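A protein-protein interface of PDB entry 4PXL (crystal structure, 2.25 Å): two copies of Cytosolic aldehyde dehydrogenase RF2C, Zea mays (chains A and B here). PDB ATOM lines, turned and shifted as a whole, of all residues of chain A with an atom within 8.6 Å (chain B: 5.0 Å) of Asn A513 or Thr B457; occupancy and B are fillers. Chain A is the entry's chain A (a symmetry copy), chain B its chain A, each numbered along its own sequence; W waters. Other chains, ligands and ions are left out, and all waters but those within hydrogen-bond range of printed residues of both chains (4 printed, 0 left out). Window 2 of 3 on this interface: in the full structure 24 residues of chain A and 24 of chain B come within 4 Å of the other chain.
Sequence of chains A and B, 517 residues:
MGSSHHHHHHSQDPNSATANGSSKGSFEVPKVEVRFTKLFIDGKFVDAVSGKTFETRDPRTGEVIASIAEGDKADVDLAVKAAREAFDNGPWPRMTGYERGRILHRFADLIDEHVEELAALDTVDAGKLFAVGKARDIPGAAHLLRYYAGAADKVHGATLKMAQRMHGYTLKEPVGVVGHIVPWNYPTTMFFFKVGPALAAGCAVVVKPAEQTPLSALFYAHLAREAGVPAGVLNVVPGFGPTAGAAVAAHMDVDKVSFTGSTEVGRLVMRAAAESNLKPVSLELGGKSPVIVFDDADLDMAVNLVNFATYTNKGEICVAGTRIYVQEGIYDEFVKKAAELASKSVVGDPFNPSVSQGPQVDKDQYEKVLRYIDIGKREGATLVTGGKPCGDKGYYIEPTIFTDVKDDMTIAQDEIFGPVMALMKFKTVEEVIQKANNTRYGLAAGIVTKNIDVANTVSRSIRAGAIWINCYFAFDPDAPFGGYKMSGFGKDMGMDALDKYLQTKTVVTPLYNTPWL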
ATOM      1  N   ARG A 165      26.194  -5.146  15.789  1.00  0.00           N
ATOM      2  CA  ARG A 165      26.048  -3.899  15.022  1.00  0.00           C
ATOM      3  C   ARG A 165      27.352  -3.115  15.197  1.00  0.00           C
ATOM      4  O   ARG A 165      27.419  -2.133  15.931  1.00  0.00           O
ATOM      5  CB  ARG A 165      24.793  -3.127  15.480  1.00  0.00           C
ATOM      6  CG  ARG A 165      24.020  -2.510  14.325  1.00  0.00           C
ATOM      7  CD  ARG A 165      22.676  -1.935  14.740  1.00  0.00           C
ATOM      8  NE  ARG A 165      21.737  -2.963  15.188  1.00  0.00           N
ATOM      9  CZ  ARG A 165      20.449  -2.742  15.440  1.00  0.00           C
ATOM     10  NH1 ARG A 165      19.928  -1.530  15.272  1.00  0.00           N
ATOM     11  NH2 ARG A 165      19.666  -3.732  15.851  1.00  0.00           N
ATOM     12  N   PRO A 510      31.353   0.538  17.175  1.00  0.00           N
ATOM     13  CA  PRO A 510      29.931   0.233  16.916  1.00  0.00           C
ATOM     14  C   PRO A 510      29.426   0.978  15.679  1.00  0.00           C
ATOM     15  O   PRO A 510      30.054   1.912  15.228  1.00  0.00           O
ATOM     16  CB  PRO A 510      29.200   0.723  18.169  1.00  0.00           C
ATOM     17  CG  PRO A 510      30.207   1.352  19.024  1.00  0.00           C
ATOM     18  CD  PRO A 510      31.518   1.422  18.340  1.00  0.00           C
ATOM     19  N   LEU A 511      28.281   0.583  15.173  1.00  0.00           N
ATOM     20  CA  LEU A 511      27.641   1.214  14.026  1.00  0.00           C
ATOM     21  C   LEU A 511      26.284   1.661  14.457  1.00  0.00           C
ATOM     22  O   LEU A 511      25.682   1.022  15.326  1.00  0.00           O
ATOM     23  CB  LEU A 511      27.476   0.217  12.884  1.00  0.00           C
ATOM     24  CG  LEU A 511      28.696  -0.118  12.101  1.00  0.00           C
ATOM     25  CD1 LEU A 511      28.396  -1.277  11.147  1.00  0.00           C
ATOM     26  CD2 LEU A 511      29.259   1.116  11.385  1.00  0.00           C
ATOM     27  N   TYR A 512      25.784   2.728  13.831  1.00  0.00           N
ATOM     28  CA  TYR A 512      24.471   3.294  14.137  1.00  0.00           C
ATOM     29  C   TYR A 512      23.666   3.467  12.848  1.00  0.00           C
ATOM     30  O   TYR A 512      24.175   4.010  11.863  1.00  0.00           O
ATOM     31  CB  TYR A 512      24.639   4.654  14.865  1.00  0.00           C
ATOM     32  CG  TYR A 512      25.447   4.536  16.147  1.00  0.00           C
ATOM     33  CD1 TYR A 512      24.859   4.088  17.324  1.00  0.00           C
ATOM     34  CD2 TYR A 512      26.811   4.810  16.161  1.00  0.00           C
ATOM     35  CE1 TYR A 512      25.606   3.914  18.486  1.00  0.00           C
ATOM     36  CE2 TYR A 512      27.575   4.613  17.312  1.00  0.00           C
ATOM     37  CZ  TYR A 512      26.963   4.190  18.480  1.00  0.00           C
ATOM     38  OH  TYR A 512      27.693   4.040  19.638  1.00  0.00           O
ATOM     39  N   ASN A 513      22.405   3.068  12.874  1.00  0.00           N
ATOM     40  CA  ASN A 513      21.478   3.213  11.734  1.00  0.00           C
ATOM     41  C   ASN A 513      22.043   2.690  10.414  1.00  0.00           C
ATOM     42  O   ASN A 513      22.020   3.384   9.401  1.00  0.00           O
ATOM     43  CB  ASN A 513      21.009   4.673  11.581  1.00  0.00           C
ATOM     44  CG  ASN A 513      20.280   5.210  12.781  1.00  0.00           C
ATOM     45  OD1 ASN A 513      19.294   4.631  13.254  1.00  0.00           O
ATOM     46  ND2 ASN A 513      20.764   6.334  13.303  1.00  0.00           N
ATOM     47  N   THR A 514      22.604   1.494  10.434  1.00  0.00           N
ATOM     48  CA  THR A 514      23.139   0.923   9.215  1.00  0.00           C
ATOM     49  C   THR A 514      22.022   0.264   8.398  1.00  0.00           C
ATOM     50  O   THR A 514      21.223  -0.482   8.977  1.00  0.00           O
ATOM     51  CB  THR A 514      24.410   0.087   9.463  1.00  0.00           C
ATOM     52  OG1 THR A 514      24.977  -0.241   8.207  1.00  0.00           O
ATOM     53  CG2 THR A 514      24.170  -1.181  10.266  1.00  0.00           C
ATOM     54  N   PRO A 515      21.897   0.576   7.079  1.00  0.00           N
ATOM     55  CA  PRO A 515      20.852  -0.087   6.259  1.00  0.00           C
ATOM     56  C   PRO A 515      21.175  -1.553   5.870  1.00  0.00           C
ATOM     57  O   PRO A 515      20.341  -2.247   5.299  1.00  0.00           O
ATOM     58  CB  PRO A 515      20.743   0.825   5.028  1.00  0.00           C
ATOM     59  CG  PRO A 515      22.122   1.381   4.872  1.00  0.00           C
ATOM     60  CD  PRO A 515      22.739   1.473   6.259  1.00  0.00           C
ATOM     61  N   TRP A 516      22.378  -2.017   6.169  1.00  0.00           N
ATOM     62  CA  TRP A 516      22.835  -3.382   5.894  1.00  0.00           C
ATOM     63  C   TRP A 516      23.920  -3.724   6.897  1.00  0.00           C
ATOM     64  O   TRP A 516      24.645  -2.836   7.354  1.00  0.00           O
ATOM     65  CB  TRP A 516      23.366  -3.539   4.445  1.00  0.00           C
ATOM     66  CG  TRP A 516      24.616  -2.744   4.164  1.00  0.00           C
ATOM     67  CD1 TRP A 516      24.689  -1.458   3.710  1.00  0.00           C
ATOM     68  CD2 TRP A 516      25.974  -3.192   4.328  1.00  0.00           C
ATOM     69  NE1 TRP A 516      26.005  -1.083   3.565  1.00  0.00           N
ATOM     70  CE2 TRP A 516      26.815  -2.110   3.979  1.00  0.00           C
ATOM     71  CE3 TRP A 516      26.559  -4.397   4.774  1.00  0.00           C
ATOM     72  CZ2 TRP A 516      28.209  -2.195   4.049  1.00  0.00           C
ATOM     73  CZ3 TRP A 516      27.943  -4.489   4.820  1.00  0.00           C
ATOM     74  CH2 TRP A 516      28.753  -3.401   4.452  1.00  0.00           C
ATOM     75  N   LEU A 517      24.089  -5.023   7.167  1.00  0.00           N
ATOM     76  CA  LEU A 517      25.106  -5.539   8.087  1.00  0.00           C
ATOM     77  C   LEU A 517      25.638  -6.877   7.521  1.00  0.00           C
ATOM     78  O   LEU A 517      24.830  -7.630   6.917  1.00  0.00           O
ATOM     79  CB  LEU A 517      24.442  -5.732   9.463  1.00  0.00           C
ATOM     80  CG  LEU A 517      25.318  -5.854  10.703  1.00  0.00           C
ATOM     81  CD1 LEU A 517      26.292  -4.658  10.855  1.00  0.00           C
ATOM     82  CD2 LEU A 517      24.437  -6.013  11.929  1.00  0.00           C
ATOM     83  OXT LEU A 517      26.867  -7.143   7.633  1.00  0.00           O
ATOM     84  N   VAL B 429      20.627  14.131   8.728  1.00  0.00           N
ATOM     85  CA  VAL B 429      21.403  13.015   8.168  1.00  0.00           C
ATOM     86  C   VAL B 429      20.480  12.128   7.269  1.00  0.00           C
ATOM     87  O   VAL B 429      20.838  11.823   6.134  1.00  0.00           O
ATOM     88  CB  VAL B 429      22.054  12.178   9.300  1.00  0.00           C
ATOM     89  CG1 VAL B 429      22.728  10.928   8.754  1.00  0.00           C
ATOM     90  CG2 VAL B 429      23.036  13.022  10.117  1.00  0.00           C
ATOM     91  N   GLU B 430      19.297  11.748   7.790  1.00  0.00           N
ATOM     92  CA  GLU B 430      18.320  10.878   7.134  1.00  0.00           C
ATOM     93  C   GLU B 430      17.851  11.490   5.833  1.00  0.00           C
ATOM     94  O   GLU B 430      17.720  10.784   4.849  1.00  0.00           O
ATOM     95  CB  GLU B 430      17.113  10.600   8.061  1.00  0.00           C
ATOM     96  CG  GLU B 430      17.469   9.913   9.382  1.00  0.00           C
ATOM     97  CD  GLU B 430      18.277  10.667  10.438  1.00  0.00           C
ATOM     98  OE1 GLU B 430      18.204  11.919  10.494  1.00  0.00           O
ATOM     99  OE2 GLU B 430      18.982   9.988  11.222  1.00  0.00           O
ATOM    100  N   ILE B 433      20.849  11.518   3.175  1.00  0.00           N
ATOM    101  CA  ILE B 433      21.082  10.176   2.649  1.00  0.00           C
ATOM    102  C   ILE B 433      20.109   9.944   1.500  1.00  0.00           C
ATOM    103  O   ILE B 433      20.536   9.469   0.441  1.00  0.00           O
ATOM    104  CB  ILE B 433      20.967   9.097   3.763  1.00  0.00           C
ATOM    105  CG1 ILE B 433      22.232   9.072   4.678  1.00  0.00           C
ATOM    106  CG2 ILE B 433      20.703   7.716   3.177  1.00  0.00           C
ATOM    107  CD1 ILE B 433      21.994   8.438   6.018  1.00  0.00           C
ATOM    108  N   ASP B 453      30.843   8.512  13.770  1.00  0.00           N
ATOM    109  CA  ASP B 453      29.526   7.891  13.623  1.00  0.00           C
ATOM    110  C   ASP B 453      28.750   8.399  12.409  1.00  0.00           C
ATOM    111  O   ASP B 453      28.209   7.598  11.661  1.00  0.00           O
ATOM    112  CB  ASP B 453      28.716   8.024  14.931  1.00  0.00           C
ATOM    113  CG  ASP B 453      29.359   7.304  16.109  1.00  0.00           C
ATOM    114  OD1 ASP B 453      29.951   6.218  15.895  1.00  0.00           O
ATOM    115  OD2 ASP B 453      29.277   7.827  17.242  1.00  0.00           O
ATOM    116  N   VAL B 454      28.715   9.717  12.196  1.00  0.00           N
ATOM    117  CA  VAL B 454      28.084  10.295  11.004  1.00  0.00           C
ATOM    118  C   VAL B 454      28.808   9.754   9.764  1.00  0.00           C
ATOM    119  O   VAL B 454      28.149   9.305   8.825  1.00  0.00           O
ATOM    120  CB  VAL B 454      28.072  11.842  11.026  1.00  0.00           C
ATOM    121  CG1 VAL B 454      27.533  12.418   9.724  1.00  0.00           C
ATOM    122  CG2 VAL B 454      27.293  12.363  12.240  1.00  0.00           C
ATOM    123  N   ALA B 455      30.154   9.783   9.766  1.00  0.00           N
ATOM    124  CA  ALA B 455      30.946   9.303   8.629  1.00  0.00           C
ATOM    125  C   ALA B 455      30.631   7.839   8.300  1.00  0.00           C
ATOM    126  O   ALA B 455      30.368   7.526   7.133  1.00  0.00           O
ATOM    127  CB  ALA B 455      32.426   9.487   8.898  1.00  0.00           C
ATOM    128  N   ASN B 456      30.558   6.967   9.334  1.00  0.00           N
ATOM    129  CA  ASN B 456      30.214   5.551   9.133  1.00  0.00           C
ATOM    130  C   ASN B 456      28.800   5.337   8.665  1.00  0.00           C
ATOM    131  O   ASN B 456      28.608   4.543   7.750  1.00  0.00           O
ATOM    132  CB  ASN B 456      30.500   4.707  10.365  1.00  0.00           C
ATOM    133  CG  ASN B 456      31.971   4.436  10.589  1.00  0.00           C
ATOM    134  OD1 ASN B 456      32.794   4.523   9.671  1.00  0.00           O
ATOM    135  ND2 ASN B 456      32.328   4.092  11.823  1.00  0.00           N
ATOM    136  N   THR B 457      27.812   6.031   9.265  1.00  0.00           N
ATOM    137  CA  THR B 457      26.398   5.907   8.875  1.00  0.00           C
ATOM    138  C   THR B 457      26.188   6.360   7.424  1.00  0.00           C
ATOM    139  O   THR B 457      25.594   5.632   6.635  1.00  0.00           O
ATOM    140  CB  THR B 457      25.471   6.639   9.870  1.00  0.00           C
ATOM    141  OG1 THR B 457      25.680   6.094  11.172  1.00  0.00           O
ATOM    142  CG2 THR B 457      23.973   6.538   9.486  1.00  0.00           C
ATOM    143  N   VAL B 458      26.688   7.554   7.084  1.00  0.00           N
ATOM    144  CA  VAL B 458      26.538   8.143   5.756  1.00  0.00           C
ATOM    145  C   VAL B 458      27.239   7.332   4.672  1.00  0.00           C
ATOM    146  O   VAL B 458      26.597   7.033   3.655  1.00  0.00           O
ATOM    147  CB  VAL B 458      26.866   9.661   5.759  1.00  0.00           C
ATOM    148  CG1 VAL B 458      26.736  10.280   4.370  1.00  0.00           C
ATOM    149  CG2 VAL B 458      25.949  10.394   6.735  1.00  0.00           C
ATOM    150  N   SER B 459      28.518   6.927   4.896  1.00  0.00           N
ATOM    151  CA  SER B 459      29.298   6.142   3.917  1.00  0.00           C
ATOM    152  C   SER B 459      28.675   4.790   3.586  1.00  0.00           C
ATOM    153  O   SER B 459      28.687   4.389   2.430  1.00  0.00           O
ATOM    154  CB  SER B 459      30.742   5.947   4.373  1.00  0.00           C
ATOM    155  OG  SER B 459      30.826   5.269   5.613  1.00  0.00           O
ATOM    156  N   ARG B 460      28.103   4.112   4.587  1.00  0.00           N
ATOM    157  CA  ARG B 460      27.458   2.830   4.386  1.00  0.00           C
ATOM    158  C   ARG B 460      26.108   2.944   3.693  1.00  0.00           C
ATOM    159  O   ARG B 460      25.661   1.988   3.080  1.00  0.00           O
ATOM    160  CB  ARG B 460      27.289   2.115   5.727  1.00  0.00           C
ATOM    161  CG  ARG B 460      28.602   1.595   6.293  1.00  0.00           C
ATOM    162  CD  ARG B 460      28.398   1.167   7.749  1.00  0.00           C
ATOM    163  NE  ARG B 460      27.749  -0.141   7.830  1.00  0.00           N
ATOM    164  CZ  ARG B 460      28.370  -1.315   7.687  1.00  0.00           C
ATOM    165  NH1 ARG B 460      29.695  -1.365   7.529  1.00  0.00           N
ATOM    166  NH2 ARG B 460      27.683  -2.448   7.764  1.00  0.00           N
ATOM    167  N   SER B 461      25.463   4.104   3.796  1.00  0.00           N
ATOM    168  CA  SER B 461      24.110   4.395   3.278  1.00  0.00           C
ATOM    169  C   SER B 461      24.046   4.974   1.864  1.00  0.00           C
ATOM    170  O   SER B 461      22.998   4.896   1.221  1.00  0.00           O
ATOM    171  CB  SER B 461      23.372   5.300   4.259  1.00  0.00           C
ATOM    172  OG  SER B 461      23.399   4.712   5.546  1.00  0.00           O
HETATM  173  O   HOH W   1      30.244   4.190  13.690  1.00  0.00           O
HETATM  174  O   HOH W   2      27.777   4.293  12.516  1.00  0.00           O
HETATM  175  O   HOH W   3      29.978   5.579  19.162  1.00  0.00           O
HETATM  176  O   HOH W   4      28.954  -5.387   7.950  1.00  0.00           O
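OG1 of Thr B457 lies within hydrogen-bond range of O of Tyr A512, at 2.7 Å.
The guanidinium group of Arg B460 is in hydrogen-bond range of the side-chain hydroxyl of Thr A514, at 2.8 Å.
NH2 of Arg B460 is in hydrogen-bond range of O of Trp A516, 3.1 Å away.
The backbone carbonyl oxygen (O) of Asp B453 lies within hydrogen-bond range of the side-chain hydroxyl (OG1) of Thr B457.
The side-chain hydroxyl of Ser B459 is in hydrogen-bond range of the backbone carbonyl oxygen of Asn B456, at 3.2 Å.
The backbone carbonyl oxygen (O) of Thr B457 lies within hydrogen-bond range of the side-chain hydroxyl (OG) of Ser B461 (2.6 Å).
The backbone carbonyl oxygen (O) of Arg A165 lies within hydrogen-bond range of the backbone NH (N) of Leu A511.
The backbone carbonyl oxygen (O) of Trp A516 lies within hydrogen-bond range of the side-chain hydroxyl (OG1) of Thr A514 (2.8 Å).
Among the printed residues, pairs that only touch across the chains: Leu A511 with Asn B456, Leu A511 with Arg B460, Tyr A512 with Asp B453, Asn A513 with Thr B457 and Pro A515 with Ser B461.
Of chain B, only Thr B457 (3.7 Å) comes within 4 Å of Asn A513.
Printed residues of chain B within 4 Å of Tyr A512: Asp B453 (3.2 Å) and Thr B457 (2.7 Å).
Of the printed residues of chain B, Trp A516 touches Arg B460.
Leu A517 touches none of the printed residues of chain B.
Hydrophobic or aromatic side chains of chain A within 4 Å of the printed part of chain B: Leu A511, Tyr A512, Pro A515 and Trp A516.
Along chain A the printed residues that touch a printed residue of chain B span positions 511 to 516.
Among the printed residues, 8 pairs touch across the chains.
Among the printed residues, no Asp or Glu carboxylate lies within 4 Å of a Lys or Arg side-chain nitrogen of the other chain.
No position is printed for both chains.
Of the 8 pairs that touch across the chains among the printed residues, none has its exchanged pair printed and touching as well.
Water W4 bridges the chain-end carboxylate (OXT) of Leu A517 (2.7 Å) and the guanidinium group (NH2) of Arg B460 (3.2 Å).
Water W1 lies within hydrogen-bond range of O of Pro A510, ND2 of Asn B456 and OD1 of Asp B453.
Water W3 lies within hydrogen-bond range of the side-chain hydroxyl (OH) of Tyr A512 and the side-chain carboxylate (OD2) of Asp B453.
Water W2 lies within hydrogen-bond range of the backbone NH (N) of Tyr A512 (2.9 Å), the side-chain hydroxyl (OG1) of Thr B457 (3.1 Å) and the backbone carbonyl oxygen (O) of Asp B453 (3.4 Å).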
